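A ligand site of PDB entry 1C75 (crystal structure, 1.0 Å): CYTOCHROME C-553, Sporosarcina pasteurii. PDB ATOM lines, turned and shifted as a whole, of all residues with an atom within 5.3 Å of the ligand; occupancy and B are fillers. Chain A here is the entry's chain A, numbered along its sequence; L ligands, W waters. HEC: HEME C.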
ATOM      1  N   VAL A   7      10.632  -3.264 -21.821  1.00  0.00           N
ATOM      2  CA  VAL A   7      12.016  -2.807 -21.559  1.00  0.00           C
ATOM      3  C   VAL A   7      12.033  -1.275 -21.462  1.00  0.00           C
ATOM      4  O   VAL A   7      12.700  -0.723 -20.579  1.00  0.00           O
ATOM      5  CB  VAL A   7      12.959  -3.334 -22.650  1.00  0.00           C
ATOM      6  CG1 VAL A   7      14.347  -2.648 -22.608  1.00  0.00           C
ATOM      7  CG2 VAL A   7      13.124  -4.848 -22.501  1.00  0.00           C
ATOM      8  N   LYS A  10      10.510  -0.394 -18.072  1.00  0.00           N
ATOM      9  CA  LYS A  10      10.997  -0.927 -16.820  1.00  0.00           C
ATOM     10  C   LYS A  10      12.518  -0.992 -16.669  1.00  0.00           C
ATOM     11  O   LYS A  10      13.010  -1.231 -15.567  1.00  0.00           O
ATOM     12  CB  LYS A  10      10.444  -2.356 -16.591  1.00  0.00           C
ATOM     13  CG  LYS A  10       8.956  -2.370 -16.460  1.00  0.00           C
ATOM     14  CD  LYS A  10       8.527  -3.751 -15.862  1.00  0.00           C
ATOM     15  CE  LYS A  10       7.058  -3.787 -15.430  1.00  0.00           C
ATOM     16  NZ  LYS A  10       6.731  -5.141 -14.940  1.00  0.00           N
ATOM     17  N   CYS A  11      13.272  -0.843 -17.769  1.00  0.00           N
ATOM     18  CA  CYS A  11      14.701  -1.149 -17.709  1.00  0.00           C
ATOM     19  C   CYS A  11      15.580   0.032 -17.997  1.00  0.00           C
ATOM     20  O   CYS A  11      16.776   0.026 -17.628  1.00  0.00           O
ATOM     21  CB  CYS A  11      15.081  -2.295 -18.678  1.00  0.00           C
ATOM     22  SG  CYS A  11      13.961  -3.713 -18.636  1.00  0.00           S
ATOM     23  N   SER A  13      15.643   3.174 -17.000  1.00  0.00           N
ATOM     24  CA  SER A  13      16.023   4.107 -15.979  1.00  0.00           C
ATOM     25  C   SER A  13      17.440   3.830 -15.491  1.00  0.00           C
ATOM     26  O   SER A  13      18.131   4.739 -15.124  1.00  0.00           O
ATOM     27  CB  SER A  13      15.080   4.046 -14.772  1.00  0.00           C
ATOM     28  OG  SER A  13      15.056   2.707 -14.274  1.00  0.00           O
ATOM     29  N   CYS A  14      17.853   2.586 -15.509  1.00  0.00           N
ATOM     30  CA  CYS A  14      19.224   2.189 -15.139  1.00  0.00           C
ATOM     31  C   CYS A  14      20.094   1.892 -16.358  1.00  0.00           C
ATOM     32  O   CYS A  14      21.298   2.156 -16.337  1.00  0.00           O
ATOM     33  CB  CYS A  14      19.229   0.990 -14.195  1.00  0.00           C
ATOM     34  SG  CYS A  14      18.277   1.418 -12.696  1.00  0.00           S
ATOM     35  N   HIS A  15      19.539   1.290 -17.405  1.00  0.00           N
ATOM     36  CA  HIS A  15      20.328   0.791 -18.519  1.00  0.00           C
ATOM     37  C   HIS A  15      20.399   1.718 -19.738  1.00  0.00           C
ATOM     38  O   HIS A  15      21.124   1.386 -20.674  1.00  0.00           O
ATOM     39  CB  HIS A  15      19.861  -0.608 -18.930  1.00  0.00           C
ATOM     40  CG  HIS A  15      20.148  -1.653 -17.891  1.00  0.00           C
ATOM     41  ND1 HIS A  15      21.413  -2.023 -17.579  1.00  0.00           N
ATOM     42  CD2 HIS A  15      19.347  -2.382 -17.078  1.00  0.00           C
ATOM     43  CE1 HIS A  15      21.373  -2.984 -16.640  1.00  0.00           C
ATOM     44  NE2 HIS A  15      20.118  -3.224 -16.318  1.00  0.00           N
ATOM     45  N   ALA A  24      23.736   1.955 -14.752  1.00  0.00           N
ATOM     46  CA  ALA A  24      24.064   0.556 -14.810  1.00  0.00           C
ATOM     47  C   ALA A  24      24.679   0.212 -16.192  1.00  0.00           C
ATOM     48  O   ALA A  24      24.601   0.985 -17.152  1.00  0.00           O
ATOM     49  CB  ALA A  24      22.841  -0.305 -14.540  1.00  0.00           C
ATOM     50  N   PRO A  25      25.278  -0.982 -16.318  1.00  0.00           N
ATOM     51  CA  PRO A  25      25.974  -1.364 -17.555  1.00  0.00           C
ATOM     52  C   PRO A  25      25.063  -1.498 -18.771  1.00  0.00           C
ATOM     53  O   PRO A  25      23.850  -1.666 -18.699  1.00  0.00           O
ATOM     54  CB  PRO A  25      26.647  -2.665 -17.177  1.00  0.00           C
ATOM     55  CG  PRO A  25      26.838  -2.597 -15.711  1.00  0.00           C
ATOM     56  CD  PRO A  25      25.553  -1.963 -15.248  1.00  0.00           C
ATOM     57  N   ALA A  26      25.678  -1.519 -19.957  1.00  0.00           N
ATOM     58  CA  ALA A  26      24.905  -1.781 -21.176  1.00  0.00           C
ATOM     59  C   ALA A  26      24.301  -3.188 -21.166  1.00  0.00           C
ATOM     60  O   ALA A  26      24.881  -4.135 -20.645  1.00  0.00           O
ATOM     61  CB  ALA A  26      25.845  -1.705 -22.367  1.00  0.00           C
ATOM     62  N   ILE A  27      23.103  -3.289 -21.783  1.00  0.00           N
ATOM     63  CA  ILE A  27      22.455  -4.552 -22.058  1.00  0.00           C
ATOM     64  C   ILE A  27      22.058  -4.709 -23.505  1.00  0.00           C
ATOM     65  O   ILE A  27      21.379  -5.683 -23.870  1.00  0.00           O
ATOM     66  CB  ILE A  27      21.225  -4.793 -21.141  1.00  0.00           C
ATOM     67  CG1 ILE A  27      20.101  -3.792 -21.367  1.00  0.00           C
ATOM     68  CG2 ILE A  27      21.674  -4.837 -19.684  1.00  0.00           C
ATOM     69  CD1 ILE A  27      18.805  -4.127 -20.654  1.00  0.00           C
ATOM     70  N   ALA A  30      23.200  -8.019 -24.745  1.00  0.00           N
ATOM     71  CA  ALA A  30      23.267  -8.998 -23.657  1.00  0.00           C
ATOM     72  C   ALA A  30      23.284 -10.433 -24.130  1.00  0.00           C
ATOM     73  O   ALA A  30      23.888 -11.291 -23.465  1.00  0.00           O
ATOM     74  CB  ALA A  30      22.126  -8.776 -22.689  1.00  0.00           C
ATOM     75  N   TYR A  34      25.204 -13.632 -22.357  1.00  0.00           N
ATOM     76  CA  TYR A  34      24.343 -14.411 -21.483  1.00  0.00           C
ATOM     77  C   TYR A  34      23.391 -15.260 -22.312  1.00  0.00           C
ATOM     78  O   TYR A  34      22.941 -14.826 -23.367  1.00  0.00           O
ATOM     79  CB  TYR A  34      23.459 -13.442 -20.602  1.00  0.00           C
ATOM     80  CG  TYR A  34      24.293 -12.606 -19.688  1.00  0.00           C
ATOM     81  CD1 TYR A  34      24.809 -11.380 -20.102  1.00  0.00           C
ATOM     82  CD2 TYR A  34      24.634 -13.010 -18.385  1.00  0.00           C
ATOM     83  CE1 TYR A  34      25.578 -10.582 -19.301  1.00  0.00           C
ATOM     84  CE2 TYR A  34      25.414 -12.232 -17.582  1.00  0.00           C
ATOM     85  CZ  TYR A  34      25.904 -11.025 -18.033  1.00  0.00           C
ATOM     86  OH  TYR A  34      26.750 -10.231 -17.257  1.00  0.00           O
ATOM     87  N   ILE A  39      19.578 -14.590 -18.498  1.00  0.00           N
ATOM     88  CA  ILE A  39      18.896 -13.311 -18.518  1.00  0.00           C
ATOM     89  C   ILE A  39      17.594 -13.398 -17.713  1.00  0.00           C
ATOM     90  O   ILE A  39      17.277 -12.478 -16.947  1.00  0.00           O
ATOM     91  CB  ILE A  39      18.649 -12.821 -19.968  1.00  0.00           C
ATOM     92  CG1 ILE A  39      20.005 -12.564 -20.659  1.00  0.00           C
ATOM     93  CG2 ILE A  39      17.784 -11.597 -19.949  1.00  0.00           C
ATOM     94  CD1 ILE A  39      19.888 -12.444 -22.173  1.00  0.00           C
ATOM     95  N   ILE A  42      18.381 -13.234 -14.029  1.00  0.00           N
ATOM     96  CA  ILE A  42      18.702 -11.869 -13.648  1.00  0.00           C
ATOM     97  C   ILE A  42      17.452 -10.997 -13.508  1.00  0.00           C
ATOM     98  O   ILE A  42      17.324 -10.241 -12.551  1.00  0.00           O
ATOM     99  CB  ILE A  42      19.697 -11.248 -14.653  1.00  0.00           C
ATOM    100  CG1 ILE A  42      21.086 -11.927 -14.534  1.00  0.00           C
ATOM    101  CG2 ILE A  42      19.794  -9.750 -14.477  1.00  0.00           C
ATOM    102  CD1 ILE A  42      21.978 -11.713 -15.717  1.00  0.00           C
ATOM    103  N   ILE A  43      16.543 -11.100 -14.460  1.00  0.00           N
ATOM    104  CA  ILE A  43      15.328 -10.298 -14.396  1.00  0.00           C
ATOM    105  C   ILE A  43      14.500 -10.666 -13.199  1.00  0.00           C
ATOM    106  O   ILE A  43      13.989  -9.838 -12.453  1.00  0.00           O
ATOM    107  CB  ILE A  43      14.526 -10.431 -15.708  1.00  0.00           C
ATOM    108  CG1 ILE A  43      15.295  -9.852 -16.887  1.00  0.00           C
ATOM    109  CG2 ILE A  43      13.152  -9.755 -15.576  1.00  0.00           C
ATOM    110  CD1 ILE A  43      14.718 -10.211 -18.241  1.00  0.00           C
ATOM    111  N   GLN A  47      20.830  -9.459  -9.587  1.00  0.00           N
ATOM    112  CA  GLN A  47      22.215  -9.969  -9.664  1.00  0.00           C
ATOM    113  C   GLN A  47      23.085  -8.824  -9.305  1.00  0.00           C
ATOM    114  O   GLN A  47      22.997  -7.735  -9.864  1.00  0.00           O
ATOM    115  CB  GLN A  47      22.593 -10.480 -11.064  1.00  0.00           C
ATOM    116  CG  GLN A  47      24.010 -11.138 -11.144  1.00  0.00           C
ATOM    117  CD  GLN A  47      24.103 -12.114 -12.303  1.00  0.00           C
ATOM    118  OE1 GLN A  47      24.751 -11.990 -13.303  1.00  0.00           O
ATOM    119  NE2 GLN A  47      23.416 -13.302 -12.262  1.00  0.00           N
ATOM    120  N   GLY A  48      23.984  -9.014  -8.323  1.00  0.00           N
ATOM    121  CA  GLY A  48      24.904  -7.944  -7.902  1.00  0.00           C
ATOM    122  C   GLY A  48      24.078  -6.715  -7.518  1.00  0.00           C
ATOM    123  O   GLY A  48      23.141  -6.773  -6.707  1.00  0.00           O
ATOM    124  N   GLY A  49      24.338  -5.552  -8.086  1.00  0.00           N
ATOM    125  CA  GLY A  49      23.672  -4.345  -7.859  1.00  0.00           C
ATOM    126  C   GLY A  49      22.259  -4.247  -8.411  1.00  0.00           C
ATOM    127  O   GLY A  49      21.583  -3.275  -8.097  1.00  0.00           O
ATOM    128  N   MET A  50      21.822  -5.153  -9.243  1.00  0.00           N
ATOM    129  CA  MET A  50      20.447  -5.092  -9.809  1.00  0.00           C
ATOM    130  C   MET A  50      19.461  -5.744  -8.860  1.00  0.00           C
ATOM    131  O   MET A  50      19.659  -6.918  -8.494  1.00  0.00           O
ATOM    132  CB  MET A  50      20.388  -5.799 -11.130  1.00  0.00           C
ATOM    133  CG  MET A  50      19.053  -5.657 -11.798  1.00  0.00           C
ATOM    134  SD  MET A  50      19.066  -6.311 -13.488  1.00  0.00           S
ATOM    135  CE  MET A  50      17.338  -6.789 -13.642  1.00  0.00           C
ATOM    136  N   PRO A  51      18.358  -5.111  -8.526  1.00  0.00           N
ATOM    137  CA  PRO A  51      17.316  -5.775  -7.689  1.00  0.00           C
ATOM    138  C   PRO A  51      16.565  -6.814  -8.473  1.00  0.00           C
ATOM    139  O   PRO A  51      16.505  -6.754  -9.701  1.00  0.00           O
ATOM    140  CB  PRO A  51      16.401  -4.594  -7.331  1.00  0.00           C
ATOM    141  CG  PRO A  51      17.062  -3.296  -7.694  1.00  0.00           C
ATOM    142  CD  PRO A  51      18.035  -3.675  -8.810  1.00  0.00           C
ATOM    143  N   ILE A  54      11.713  -6.920 -10.880  1.00  0.00           N
ATOM    144  CA  ILE A  54      11.264  -5.840 -11.713  1.00  0.00           C
ATOM    145  C   ILE A  54      10.304  -6.303 -12.790  1.00  0.00           C
ATOM    146  O   ILE A  54       9.326  -5.556 -13.127  1.00  0.00           O
ATOM    147  CB  ILE A  54      12.477  -5.107 -12.355  1.00  0.00           C
ATOM    148  CG1 ILE A  54      13.275  -4.419 -11.255  1.00  0.00           C
ATOM    149  CG2 ILE A  54      12.042  -4.128 -13.408  1.00  0.00           C
ATOM    150  CD1 ILE A  54      14.678  -3.966 -11.643  1.00  0.00           C
ATOM    151  N   ALA A  55      10.454  -7.522 -13.298  1.00  0.00           N
ATOM    152  CA  ALA A  55       9.458  -8.156 -14.160  1.00  0.00           C
ATOM    153  C   ALA A  55       9.311  -9.610 -13.754  1.00  0.00           C
ATOM    154  O   ALA A  55      10.210 -10.156 -13.087  1.00  0.00           O
ATOM    155  CB  ALA A  55       9.785  -8.001 -15.635  1.00  0.00           C
ATOM    156  N   VAL A  63      10.872 -10.748 -22.340  1.00  0.00           N
ATOM    157  CA  VAL A  63      12.032  -9.853 -22.327  1.00  0.00           C
ATOM    158  C   VAL A  63      13.320 -10.643 -22.433  1.00  0.00           C
ATOM    159  O   VAL A  63      14.218 -10.255 -23.186  1.00  0.00           O
ATOM    160  CB  VAL A  63      11.995  -8.895 -21.097  1.00  0.00           C
ATOM    161  CG1 VAL A  63      13.307  -8.131 -20.980  1.00  0.00           C
ATOM    162  CG2 VAL A  63      10.827  -7.967 -21.184  1.00  0.00           C
ATOM    163  N   LEU A  67      16.000 -10.123 -25.471  1.00  0.00           N
ATOM    164  CA  LEU A  67      17.372  -9.730 -25.206  1.00  0.00           C
ATOM    165  C   LEU A  67      18.393 -10.782 -25.607  1.00  0.00           C
ATOM    166  O   LEU A  67      19.482 -10.497 -26.034  1.00  0.00           O
ATOM    167  CB  LEU A  67      17.627  -9.377 -23.729  1.00  0.00           C
ATOM    168  CG  LEU A  67      17.029  -8.063 -23.273  1.00  0.00           C
ATOM    169  CD1 LEU A  67      17.229  -7.979 -21.752  1.00  0.00           C
ATOM    170  CD2 LEU A  67      17.714  -6.880 -23.954  1.00  0.00           C
HETATM  171 FE   HEC L   1      19.569  -4.603 -14.990  1.00  0.00          FE
HETATM  172  CHA HEC L   1      22.669  -5.975 -14.802  1.00  0.00           C
HETATM  173  CHB HEC L   1      18.790  -6.686 -17.567  1.00  0.00           C
HETATM  174  CHC HEC L   1      16.393  -3.354 -15.037  1.00  0.00           C
HETATM  175  CHD HEC L   1      20.394  -2.308 -12.636  1.00  0.00           C
HETATM  176  NA  HEC L   1      20.535  -6.029 -16.000  1.00  0.00           N
HETATM  177  C1A HEC L   1      21.822  -6.493 -15.774  1.00  0.00           C
HETATM  178  C2A HEC L   1      22.138  -7.566 -16.675  1.00  0.00           C
HETATM  179  C3A HEC L   1      21.072  -7.730 -17.490  1.00  0.00           C
HETATM  180  C4A HEC L   1      20.065  -6.783 -17.041  1.00  0.00           C
HETATM  181  CMA HEC L   1      20.890  -8.671 -18.638  1.00  0.00           C
HETATM  182  CAA HEC L   1      23.451  -8.323 -16.696  1.00  0.00           C
HETATM  183  CBA HEC L   1      24.670  -7.474 -17.135  1.00  0.00           C
HETATM  184  CGA HEC L   1      24.555  -6.876 -18.409  1.00  0.00           C
HETATM  185  O1A HEC L   1      24.052  -7.448 -19.394  1.00  0.00           O
HETATM  186  O2A HEC L   1      24.946  -5.643 -18.483  1.00  0.00           O
HETATM  187  NB  HEC L   1      17.941  -4.960 -16.050  1.00  0.00           N
HETATM  188  C1B HEC L   1      17.790  -5.842 -17.087  1.00  0.00           C
HETATM  189  C2B HEC L   1      16.463  -5.784 -17.654  1.00  0.00           C
HETATM  190  C3B HEC L   1      15.763  -4.908 -16.901  1.00  0.00           C
HETATM  191  C4B HEC L   1      16.697  -4.370 -15.919  1.00  0.00           C
HETATM  192  CMB HEC L   1      16.037  -6.570 -18.857  1.00  0.00           C
HETATM  193  CAB HEC L   1      14.329  -4.476 -17.020  1.00  0.00           C
HETATM  194  CBB HEC L   1      13.334  -5.646 -16.845  1.00  0.00           C
HETATM  195  NC  HEC L   1      18.597  -3.183 -14.002  1.00  0.00           N
HETATM  196  C1C HEC L   1      17.266  -2.788 -14.156  1.00  0.00           C
HETATM  197  C2C HEC L   1      16.970  -1.636 -13.347  1.00  0.00           C
HETATM  198  C3C HEC L   1      18.095  -1.359 -12.669  1.00  0.00           C
HETATM  199  C4C HEC L   1      19.087  -2.301 -13.088  1.00  0.00           C
HETATM  200  CMC HEC L   1      15.656  -0.899 -13.364  1.00  0.00           C
HETATM  201  CAC HEC L   1      18.360  -0.148 -11.791  1.00  0.00           C
HETATM  202  CBC HEC L   1      17.340  -0.065 -10.618  1.00  0.00           C
HETATM  203  ND  HEC L   1      21.189  -4.221 -13.944  1.00  0.00           N
HETATM  204  C1D HEC L   1      21.376  -3.210 -13.019  1.00  0.00           C
HETATM  205  C2D HEC L   1      22.705  -3.231 -12.456  1.00  0.00           C
HETATM  206  C3D HEC L   1      23.349  -4.252 -13.080  1.00  0.00           C
HETATM  207  C4D HEC L   1      22.381  -4.879 -13.988  1.00  0.00           C
HETATM  208  CMD HEC L   1      23.160  -2.283 -11.399  1.00  0.00           C
HETATM  209  CAD HEC L   1      24.731  -4.795 -12.906  1.00  0.00           C
HETATM  210  CBD HEC L   1      24.732  -6.159 -12.098  1.00  0.00           C
HETATM  211  CGD HEC L   1      25.713  -7.049 -12.568  1.00  0.00           C
HETATM  212  O1D HEC L   1      26.781  -7.219 -11.895  1.00  0.00           O
HETATM  213  O2D HEC L   1      25.585  -7.626 -13.682  1.00  0.00           O
HETATM  214  O   HOH W   1      20.108  -1.045  -8.943  1.00  0.00           O
HETATM  215  O   HOH W   2      26.341 -10.105 -14.570  1.00  0.00           O
HETATM  216  O   HOH W   3      25.521  -7.709 -21.757  1.00  0.00           O
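Lys 10 touches the ligand (O to CMC, 3.5 Å). Ser 13 touches the ligand (OG to CMC, 3.8 Å). Ala 24 touches the ligand (CB to C1D, 3.6 Å). CB of Pro 25 touches O2A of the ligand (3.7 Å). Ile 27 touches the ligand (CG2 to O1A, 3.5 Å). Tyr 34 touches the ligand. CD1 of Ile 42 touches CAA of the ligand (3.8 Å). Ile 43 touches the ligand. O of Gln 47 touches CBD of the ligand (3.2 Å). Gly 49 touches the ligand. Ile 54 touches the ligand (CD1 to CMC, 3.7 Å). Val 63 touches the ligand (CG1 to CMB, 3.8 Å). Leu 67 touches the ligand. Hydrophobic or aromatic side chains within 4 Å of the ligand: His 15, Ala 24, Pro 25, Ile 27, Tyr 34, Ile 42, Ile 43, Met 50, Ile 54, Val 63 and Leu 67. Of the 24 residues printed, 18 come within 4 Å of the ligand. The nearest printed residue that does not touch the ligand is Ala 30 (4.04 Å).
Water W2 lies within hydrogen-bond range of the side-chain hydroxyl (OH) of Tyr 34 (2.7 Å), an oxygen (O2D) of the ligand (2.7 Å) and the side-chain amide oxygen (OE1) of Gln 47 (2.8 Å).
A carbon (CAC) of the ligand is covalently linked to the side-chain sulfur (SG) of Cys 14, 1.8 Å away. CAB of the ligand is covalently linked to SG of Cys 11 (1.8 Å). FE of the ligand is bound by NE2 of His 15, 2.0 Å away. The side-chain sulfur of Met 50 is bound to an iron atom (FE) of the ligand. The backbone carbonyl oxygen (O) of Ala 26 sits close to an oxygen (O2A) of the ligand.
O of Cys 14 is in hydrogen-bond range of N of Ala 24 (2.9 Å). ND1 of His 15 is in hydrogen-bond range of O of Pro 25, at 2.7 Å. O of Ile 54 lies within hydrogen-bond range of NZ of Lys 10 (3.2 Å).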
